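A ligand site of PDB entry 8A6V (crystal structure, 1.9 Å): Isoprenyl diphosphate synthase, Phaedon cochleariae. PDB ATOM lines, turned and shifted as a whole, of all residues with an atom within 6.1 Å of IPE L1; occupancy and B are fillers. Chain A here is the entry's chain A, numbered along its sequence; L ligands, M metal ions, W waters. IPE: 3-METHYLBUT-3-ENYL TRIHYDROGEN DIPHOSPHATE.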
ATOM      1  N   THR A  48       3.558   0.930  23.218  1.00  0.00           N
ATOM      2  CA  THR A  48       4.171   1.870  22.237  1.00  0.00           C
ATOM      3  C   THR A  48       5.379   1.238  21.531  1.00  0.00           C
ATOM      4  O   THR A  48       6.056   1.978  20.782  1.00  0.00           O
ATOM      5  CB  THR A  48       4.541   3.208  22.878  1.00  0.00           C
ATOM      6  OG1 THR A  48       5.737   3.049  23.628  1.00  0.00           O
ATOM      7  CG2 THR A  48       3.440   3.765  23.760  1.00  0.00           C
ATOM      8  N   GLY A  49       5.624  -0.059  21.727  1.00  0.00           N
ATOM      9  CA  GLY A  49       6.667  -0.815  21.007  1.00  0.00           C
ATOM     10  C   GLY A  49       6.187  -1.255  19.632  1.00  0.00           C
ATOM     11  O   GLY A  49       5.094  -0.823  19.225  1.00  0.00           O
ATOM     12  N   LYS A  50       6.973  -2.085  18.937  1.00  0.00           N
ATOM     13  CA  LYS A  50       6.631  -2.660  17.611  1.00  0.00           C
ATOM     14  C   LYS A  50       5.592  -3.771  17.802  1.00  0.00           C
ATOM     15  O   LYS A  50       4.864  -4.054  16.837  1.00  0.00           O
ATOM     16  CB  LYS A  50       7.892  -3.155  16.893  1.00  0.00           C
ATOM     17  CG  LYS A  50       8.923  -2.079  16.618  1.00  0.00           C
ATOM     18  CD  LYS A  50      10.123  -2.559  15.817  1.00  0.00           C
ATOM     19  CE  LYS A  50      10.985  -3.570  16.552  1.00  0.00           C
ATOM     20  NZ  LYS A  50      11.586  -3.008  17.778  1.00  0.00           N
ATOM     21  N   LYS A  51       5.537  -4.372  18.999  1.00  0.00           N
ATOM     22  CA  LYS A  51       4.536  -5.388  19.418  1.00  0.00           C
ATOM     23  C   LYS A  51       4.705  -6.687  18.603  1.00  0.00           C
ATOM     24  O   LYS A  51       3.704  -7.407  18.431  1.00  0.00           O
ATOM     25  CB  LYS A  51       3.114  -4.836  19.284  1.00  0.00           C
ATOM     26  CG  LYS A  51       2.771  -3.692  20.231  1.00  0.00           C
ATOM     27  CD  LYS A  51       1.443  -3.033  19.935  1.00  0.00           C
ATOM     28  CE  LYS A  51       1.524  -1.957  18.866  1.00  0.00           C
ATOM     29  NZ  LYS A  51       2.242  -0.749  19.348  1.00  0.00           N
ATOM     30  N   THR A  52       5.921  -6.975  18.145  1.00  0.00           N
ATOM     31  CA  THR A  52       6.238  -8.161  17.305  1.00  0.00           C
ATOM     32  C   THR A  52       5.972  -9.454  18.099  1.00  0.00           C
ATOM     33  O   THR A  52       5.431 -10.398  17.497  1.00  0.00           O
ATOM     34  CB  THR A  52       7.677  -8.094  16.773  1.00  0.00           C
ATOM     35  OG1 THR A  52       7.762  -6.928  15.942  1.00  0.00           O
ATOM     36  CG2 THR A  52       8.091  -9.312  15.966  1.00  0.00           C
ATOM     37  N   ARG A  53       6.317  -9.481  19.388  1.00  0.00           N
ATOM     38  CA  ARG A  53       6.123 -10.658  20.274  1.00  0.00           C
ATOM     39  C   ARG A  53       4.619 -10.949  20.408  1.00  0.00           C
ATOM     40  O   ARG A  53       4.235 -12.114  20.233  1.00  0.00           O
ATOM     41  CB  ARG A  53       6.760 -10.434  21.647  1.00  0.00           C
ATOM     42  CG  ARG A  53       8.282 -10.322  21.623  1.00  0.00           C
ATOM     43  CD  ARG A  53       8.823  -9.855  22.956  1.00  0.00           C
ATOM     44  NE  ARG A  53      10.254  -9.595  22.927  1.00  0.00           N
ATOM     45  CZ  ARG A  53      10.824  -8.536  22.346  1.00  0.00           C
ATOM     46  NH1 ARG A  53      10.084  -7.620  21.744  1.00  0.00           N
ATOM     47  NH2 ARG A  53      12.139  -8.405  22.382  1.00  0.00           N
ATOM     48  N   GLU A  86       3.596  -9.007  25.997  1.00  0.00           N
ATOM     49  CA  GLU A  86       3.937  -7.565  25.937  1.00  0.00           C
ATOM     50  C   GLU A  86       4.048  -6.997  27.364  1.00  0.00           C
ATOM     51  O   GLU A  86       4.889  -6.111  27.568  1.00  0.00           O
ATOM     52  CB  GLU A  86       2.919  -6.798  25.089  1.00  0.00           C
ATOM     53  CG  GLU A  86       3.017  -7.124  23.605  1.00  0.00           C
ATOM     54  CD  GLU A  86       4.363  -6.809  22.960  1.00  0.00           C
ATOM     55  OE1 GLU A  86       5.037  -5.868  23.437  1.00  0.00           O
ATOM     56  OE2 GLU A  86       4.725  -7.500  21.991  1.00  0.00           O
ATOM     57  N   GLN A  89       7.462  -8.146  28.439  1.00  0.00           N
ATOM     58  CA  GLN A  89       8.406  -7.251  27.702  1.00  0.00           C
ATOM     59  C   GLN A  89       8.487  -5.908  28.423  1.00  0.00           C
ATOM     60  O   GLN A  89       9.614  -5.456  28.696  1.00  0.00           O
ATOM     61  CB  GLN A  89       7.981  -7.116  26.238  1.00  0.00           C
ATOM     62  CG  GLN A  89       8.698  -6.006  25.476  1.00  0.00           C
ATOM     63  CD  GLN A  89      10.153  -6.292  25.189  1.00  0.00           C
ATOM     64  OE1 GLN A  89      10.826  -7.010  25.925  1.00  0.00           O
ATOM     65  NE2 GLN A  89      10.657  -5.715  24.109  1.00  0.00           N
ATOM     66  N   LEU A  93      11.907  -4.175  30.118  1.00  0.00           N
ATOM     67  CA  LEU A  93      12.486  -2.909  29.588  1.00  0.00           C
ATOM     68  C   LEU A  93      12.584  -1.858  30.708  1.00  0.00           C
ATOM     69  O   LEU A  93      13.627  -1.164  30.746  1.00  0.00           O
ATOM     70  CB  LEU A  93      11.640  -2.400  28.415  1.00  0.00           C
ATOM     71  CG  LEU A  93      11.598  -3.296  27.179  1.00  0.00           C
ATOM     72  CD1 LEU A  93      11.032  -2.549  25.984  1.00  0.00           C
ATOM     73  CD2 LEU A  93      12.964  -3.868  26.851  1.00  0.00           C
ATOM     74  N   ARG A 105      13.637   5.319  25.570  1.00  0.00           N
ATOM     75  CA  ARG A 105      12.995   4.034  25.199  1.00  0.00           C
ATOM     76  C   ARG A 105      11.757   4.358  24.350  1.00  0.00           C
ATOM     77  O   ARG A 105      10.929   5.157  24.824  1.00  0.00           O
ATOM     78  CB  ARG A 105      12.593   3.253  26.456  1.00  0.00           C
ATOM     79  CG  ARG A 105      11.759   2.007  26.192  1.00  0.00           C
ATOM     80  CD  ARG A 105      12.530   0.927  25.469  1.00  0.00           C
ATOM     81  NE  ARG A 105      13.592   0.362  26.288  1.00  0.00           N
ATOM     82  CZ  ARG A 105      14.439  -0.585  25.884  1.00  0.00           C
ATOM     83  NH1 ARG A 105      14.365  -1.087  24.666  1.00  0.00           N
ATOM     84  NH2 ARG A 105      15.375  -1.025  26.719  1.00  0.00           N
ATOM     85  N   ARG A 106      11.654   3.773  23.162  1.00  0.00           N
ATOM     86  CA  ARG A 106      10.485   3.945  22.248  1.00  0.00           C
ATOM     87  C   ARG A 106      10.203   5.436  22.059  1.00  0.00           C
ATOM     88  O   ARG A 106       9.013   5.830  22.114  1.00  0.00           O
ATOM     89  CB  ARG A 106       9.282   3.182  22.811  1.00  0.00           C
ATOM     90  CG  ARG A 106       9.502   1.685  22.966  1.00  0.00           C
ATOM     91  CD  ARG A 106       8.501   1.032  23.902  1.00  0.00           C
ATOM     92  NE  ARG A 106       8.540  -0.429  23.854  1.00  0.00           N
ATOM     93  CZ  ARG A 106       7.776  -1.238  24.574  1.00  0.00           C
ATOM     94  NH1 ARG A 106       6.893  -0.746  25.423  1.00  0.00           N
ATOM     95  NH2 ARG A 106       7.893  -2.551  24.449  1.00  0.00           N
ATOM     96  N   LYS A 193      18.788 -14.495  27.730  1.00  0.00           N
ATOM     97  CA  LYS A 193      18.401 -13.066  27.889  1.00  0.00           C
ATOM     98  C   LYS A 193      17.273 -12.698  26.907  1.00  0.00           C
ATOM     99  O   LYS A 193      16.379 -11.929  27.319  1.00  0.00           O
ATOM    100  CB  LYS A 193      19.620 -12.164  27.669  1.00  0.00           C
ATOM    101  CG  LYS A 193      19.402 -10.686  27.917  1.00  0.00           C
ATOM    102  CD  LYS A 193      20.619  -9.831  27.627  1.00  0.00           C
ATOM    103  CE  LYS A 193      20.704  -9.388  26.171  1.00  0.00           C
ATOM    104  NZ  LYS A 193      21.730  -8.323  25.991  1.00  0.00           N
ATOM    105  N   THR A 194      17.298 -13.211  25.672  1.00  0.00           N
ATOM    106  CA  THR A 194      16.452 -12.733  24.540  1.00  0.00           C
ATOM    107  C   THR A 194      15.605 -13.863  23.943  1.00  0.00           C
ATOM    108  O   THR A 194      14.373 -13.670  23.836  1.00  0.00           O
ATOM    109  CB  THR A 194      17.319 -12.069  23.470  1.00  0.00           C
ATOM    110  OG1 THR A 194      17.907 -10.909  24.039  1.00  0.00           O
ATOM    111  CG2 THR A 194      16.547 -11.685  22.222  1.00  0.00           C
ATOM    112  N   TYR A 197      12.170 -15.676  25.636  1.00  0.00           N
ATOM    113  CA  TYR A 197      10.975 -14.820  25.898  1.00  0.00           C
ATOM    114  C   TYR A 197      10.508 -14.141  24.607  1.00  0.00           C
ATOM    115  O   TYR A 197       9.301 -13.886  24.497  1.00  0.00           O
ATOM    116  CB  TYR A 197      11.231 -13.849  27.059  1.00  0.00           C
ATOM    117  CG  TYR A 197      11.655 -12.449  26.688  1.00  0.00           C
ATOM    118  CD1 TYR A 197      10.719 -11.455  26.474  1.00  0.00           C
ATOM    119  CD2 TYR A 197      13.000 -12.110  26.591  1.00  0.00           C
ATOM    120  CE1 TYR A 197      11.092 -10.157  26.152  1.00  0.00           C
ATOM    121  CE2 TYR A 197      13.392 -10.825  26.266  1.00  0.00           C
ATOM    122  CZ  TYR A 197      12.437  -9.842  26.051  1.00  0.00           C
ATOM    123  OH  TYR A 197      12.828  -8.575  25.739  1.00  0.00           O
ATOM    124  N   THR A 198      11.415 -13.861  23.663  1.00  0.00           N
ATOM    125  CA  THR A 198      11.111 -13.080  22.437  1.00  0.00           C
ATOM    126  C   THR A 198      10.529 -13.984  21.334  1.00  0.00           C
ATOM    127  O   THR A 198       9.633 -13.505  20.612  1.00  0.00           O
ATOM    128  CB  THR A 198      12.332 -12.296  21.945  1.00  0.00           C
ATOM    129  OG1 THR A 198      12.733 -11.428  23.010  1.00  0.00           O
ATOM    130  CG2 THR A 198      12.061 -11.480  20.706  1.00  0.00           C
ATOM    131  N   PHE A 232      18.467 -12.032  15.841  1.00  0.00           N
ATOM    132  CA  PHE A 232      17.716 -10.827  16.277  1.00  0.00           C
ATOM    133  C   PHE A 232      18.572  -9.978  17.232  1.00  0.00           C
ATOM    134  O   PHE A 232      18.556  -8.740  17.093  1.00  0.00           O
ATOM    135  CB  PHE A 232      16.382 -11.228  16.920  1.00  0.00           C
ATOM    136  CG  PHE A 232      15.584 -10.084  17.482  1.00  0.00           C
ATOM    137  CD1 PHE A 232      14.650  -9.409  16.706  1.00  0.00           C
ATOM    138  CD2 PHE A 232      15.741  -9.686  18.801  1.00  0.00           C
ATOM    139  CE1 PHE A 232      13.907  -8.362  17.220  1.00  0.00           C
ATOM    140  CE2 PHE A 232      15.003  -8.631  19.318  1.00  0.00           C
ATOM    141  CZ  PHE A 232      14.090  -7.980  18.532  1.00  0.00           C
ATOM    142  N   GLN A 233      19.278 -10.614  18.178  1.00  0.00           N
ATOM    143  CA  GLN A 233      20.060  -9.895  19.223  1.00  0.00           C
ATOM    144  C   GLN A 233      21.325  -9.310  18.603  1.00  0.00           C
ATOM    145  O   GLN A 233      21.733  -8.207  19.031  1.00  0.00           O
ATOM    146  CB  GLN A 233      20.382 -10.802  20.406  1.00  0.00           C
ATOM    147  CG  GLN A 233      21.038 -10.058  21.574  1.00  0.00           C
ATOM    148  CD  GLN A 233      20.213  -8.896  22.082  1.00  0.00           C
ATOM    149  OE1 GLN A 233      19.061  -9.058  22.473  1.00  0.00           O
ATOM    150  NE2 GLN A 233      20.808  -7.716  22.081  1.00  0.00           N
ATOM    151  N   ASP A 236      20.270  -6.188  17.104  1.00  0.00           N
ATOM    152  CA  ASP A 236      20.043  -5.207  18.202  1.00  0.00           C
ATOM    153  C   ASP A 236      21.393  -4.625  18.650  1.00  0.00           C
ATOM    154  O   ASP A 236      21.469  -3.393  18.853  1.00  0.00           O
ATOM    155  CB  ASP A 236      19.321  -5.830  19.388  1.00  0.00           C
ATOM    156  CG  ASP A 236      19.052  -4.826  20.503  1.00  0.00           C
ATOM    157  OD1 ASP A 236      18.187  -3.955  20.306  1.00  0.00           O
ATOM    158  OD2 ASP A 236      19.734  -4.911  21.547  1.00  0.00           O
ATOM    159  N   LYS A 250      15.828   4.740  20.893  1.00  0.00           N
ATOM    160  CA  LYS A 250      16.700   4.534  22.077  1.00  0.00           C
ATOM    161  C   LYS A 250      18.135   4.943  21.757  1.00  0.00           C
ATOM    162  O   LYS A 250      18.553   4.851  20.587  1.00  0.00           O
ATOM    163  CB  LYS A 250      16.599   3.084  22.566  1.00  0.00           C
ATOM    164  CG  LYS A 250      17.221   2.037  21.652  1.00  0.00           C
ATOM    165  CD  LYS A 250      16.764   0.628  21.978  1.00  0.00           C
ATOM    166  CE  LYS A 250      17.455  -0.437  21.142  1.00  0.00           C
ATOM    167  NZ  LYS A 250      16.966  -1.789  21.480  1.00  0.00           N
ATOM    168  N   ARG A 344      16.052  -5.028   9.444  1.00  0.00           N
ATOM    169  CA  ARG A 344      15.309  -4.038  10.271  1.00  0.00           C
ATOM    170  C   ARG A 344      16.281  -2.938  10.728  1.00  0.00           C
ATOM    171  O   ARG A 344      17.483  -3.251  10.889  1.00  0.00           O
ATOM    172  CB  ARG A 344      14.635  -4.714  11.468  1.00  0.00           C
ATOM    173  CG  ARG A 344      15.590  -5.265  12.524  1.00  0.00           C
ATOM    174  CD  ARG A 344      14.881  -6.162  13.506  1.00  0.00           C
ATOM    175  NE  ARG A 344      15.754  -6.576  14.596  1.00  0.00           N
ATOM    176  CZ  ARG A 344      15.882  -5.935  15.765  1.00  0.00           C
ATOM    177  NH1 ARG A 344      15.187  -4.846  16.013  1.00  0.00           N
ATOM    178  NH2 ARG A 344      16.726  -6.406  16.674  1.00  0.00           N
ATOM    179  N   ALA A 346      15.109  -0.859  13.341  1.00  0.00           N
ATOM    180  CA  ALA A 346      14.521  -0.582  14.672  1.00  0.00           C
ATOM    181  C   ALA A 346      13.961  -1.880  15.275  1.00  0.00           C
ATOM    182  O   ALA A 346      13.700  -1.940  16.475  1.00  0.00           O
ATOM    183  CB  ALA A 346      13.451   0.476  14.562  1.00  0.00           C
ATOM    184  OXT ALA A 346      13.785  -2.879  14.585  1.00  0.00           O
HETATM  185  C1  IPE L   1      14.041  -4.751  22.796  1.00  0.00           C
HETATM  186  O1  IPE L   1      13.117  -5.529  22.001  1.00  0.00           O
HETATM  187  C2  IPE L   1      14.752  -5.647  23.788  1.00  0.00           C
HETATM  188  C3  IPE L   1      15.560  -6.750  23.176  1.00  0.00           C
HETATM  189  C4  IPE L   1      15.349  -8.033  23.464  1.00  0.00           C
HETATM  190  C5  IPE L   1      16.642  -6.319  22.223  1.00  0.00           C
HETATM  191  PA  IPE L   1      12.363  -4.838  20.769  1.00  0.00           P
HETATM  192  O1A IPE L   1      13.398  -4.260  19.859  1.00  0.00           O
HETATM  193  O2A IPE L   1      11.412  -5.850  20.227  1.00  0.00           O
HETATM  194  O3A IPE L   1      11.554  -3.641  21.472  1.00  0.00           O
HETATM  195  PB  IPE L   1      10.053  -3.042  21.360  1.00  0.00           P
HETATM  196  O1B IPE L   1      10.176  -1.591  21.761  1.00  0.00           O
HETATM  197  O2B IPE L   1       9.600  -3.207  19.939  1.00  0.00           O
HETATM  198  O3B IPE L   1       9.206  -3.836  22.334  1.00  0.00           O
HETATM  199  C1  IPE L   2      17.554  -6.482  26.873  1.00  0.00           C
HETATM  200  O1  IPE L   2      18.760  -6.466  26.096  1.00  0.00           O
HETATM  201  C2  IPE L   2      16.960  -7.842  27.015  1.00  0.00           C
HETATM  202  C3  IPE L   2      15.926  -7.870  28.102  1.00  0.00           C
HETATM  203  C4  IPE L   2      15.845  -8.860  28.976  1.00  0.00           C
HETATM  204  C5  IPE L   2      15.009  -6.679  28.156  1.00  0.00           C
HETATM  205  PA  IPE L   2      19.368  -5.030  25.787  1.00  0.00           P
HETATM  206  O1A IPE L   2      20.356  -5.112  24.666  1.00  0.00           O
HETATM  207  O2A IPE L   2      19.760  -4.414  27.086  1.00  0.00           O
HETATM  208  O3A IPE L   2      18.049  -4.288  25.255  1.00  0.00           O
HETATM  209  PB  IPE L   2      17.891  -2.801  24.693  1.00  0.00           P
HETATM  210  O1B IPE L   2      18.886  -2.723  23.552  1.00  0.00           O
HETATM  211  O2B IPE L   2      16.464  -2.639  24.228  1.00  0.00           O
HETATM  212  O3B IPE L   2      18.239  -1.892  25.842  1.00  0.00           O
HETATM  213 MG    MG M   1      20.577  -3.623  22.987  1.00  0.00          MG
HETATM  214  O   HOH W   1      10.770  -6.995  18.005  1.00  0.00           O
HETATM  215  O   HOH W   2      15.926  -4.764  18.768  1.00  0.00           O
HETATM  216  O   HOH W   3      10.247  -0.056  19.509  1.00  0.00           O
HETATM  217  O   HOH W   4      12.559  -0.594  22.363  1.00  0.00           O
HETATM  218  O   HOH W   5       6.465  -4.147  21.774  1.00  0.00           O
HETATM  219  O   HOH W   6       8.449  -5.668  19.326  1.00  0.00           O
HETATM  220  O   HOH W   7      14.362  -1.851  20.513  1.00  0.00           O
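The backbone NH (N) of Lys 50 sits at hydrogen-bond distance from an oxygen (O2B) of IPE L1 (3.0 Å).
NZ of Lys 250 is in salt-bridge range of O2B of IPE L2, at 2.9 Å.
NH1 of Arg 53 is in salt-bridge range of O2A of IPE L1.
An oxygen (O3B) of IPE L1 lies within hydrogen-bond range of the side-chain amide nitrogen of Gln 89, at 3.0 Å.
The side-chain amino group of Lys 193 lies close to an oxygen (O1A) of IPE L2 (3.7 Å).
An oxygen (O2B) of IPE L1 lies within salt-bridge range of the side-chain amino group of Lys 50, 2.9 Å away.
An oxygen (O2B) of IPE L2 is in salt-bridge range of the guanidinium group of Arg 105, at 2.6 Å.
O3B of IPE L1 lies within salt-bridge range of NH2 of Arg 106, at 2.8 Å.
The side-chain amino group (NZ) of Lys 50 is in salt-bridge range of the chain-end carboxylate (O) of Ala 346 (2.7 Å).
OD2 of Asp 236 sits close to NE2 of Gln 233 (3.1 Å).
O of Phe 232 is in hydrogen-bond range of NH2 of Arg 344, 3.0 Å away.
The side-chain carboxylate (OD1) of Asp 236 is in salt-bridge range of the side-chain amino group (NZ) of Lys 250, 2.7 Å away.
The guanidinium group of Arg 53 sits close to the side-chain amide nitrogen of Gln 89, at 3.1 Å.
The side-chain hydroxyl (OG1) of Thr 194 is in hydrogen-bond range of the side-chain amide oxygen (OE1) of Gln 233.
O of Thr 194 sits at hydrogen-bond distance from OG1 of Thr 198 (2.9 Å).
The guanidinium group (NH2) of Arg 53 lies within hydrogen-bond range of the side-chain hydroxyl (OH) of Tyr 197, at 3.4 Å.
CA of Gly 49 touches O1B of IPE L1, 3.7 Å away.
Leu 93 touches IPE L1.
Thr 194 touches IPE L1 (OG1 to C4, 3.9 Å).
Tyr 197 touches IPE L1 (OH to C4, 3.4 Å).
Phe 232 touches IPE L1.
Gln 233 touches IPE L1 (OE1 to C5, 3.7 Å).
CG of Asp 236 touches C5 of IPE L1, at 3.3 Å.
Hydrophobic or aromatic side chains that line IPE L1: Leu 93 and Phe 232.
Of the 21 residues printed, 11 come within 4 Å of IPE L1.
Water W4 lies within hydrogen-bond range of O1B of IPE L1 and NH1 of Arg 105.
Water W7 bridges O1A of IPE L1 (2.7 Å) and NZ of Lys 250 (2.8 Å).
Water W6 lies within hydrogen-bond range of O2B of IPE L1 (2.8 Å), N of Thr 52 (3.1 Å) and N of Lys 51 (3.2 Å).
Water W2 lies within hydrogen-bond range of NH2 of Arg 344 (2.8 Å), O1A of IPE L1 (2.8 Å) and OD1 of Asp 236 (2.9 Å).
Water W5 lies within hydrogen-bond range of the side-chain carboxylate (OE1) of Glu 86, an oxygen (O3B) of IPE L1, the backbone NH (N) of Lys 51 and the guanidinium group (NH2) of Arg 106.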
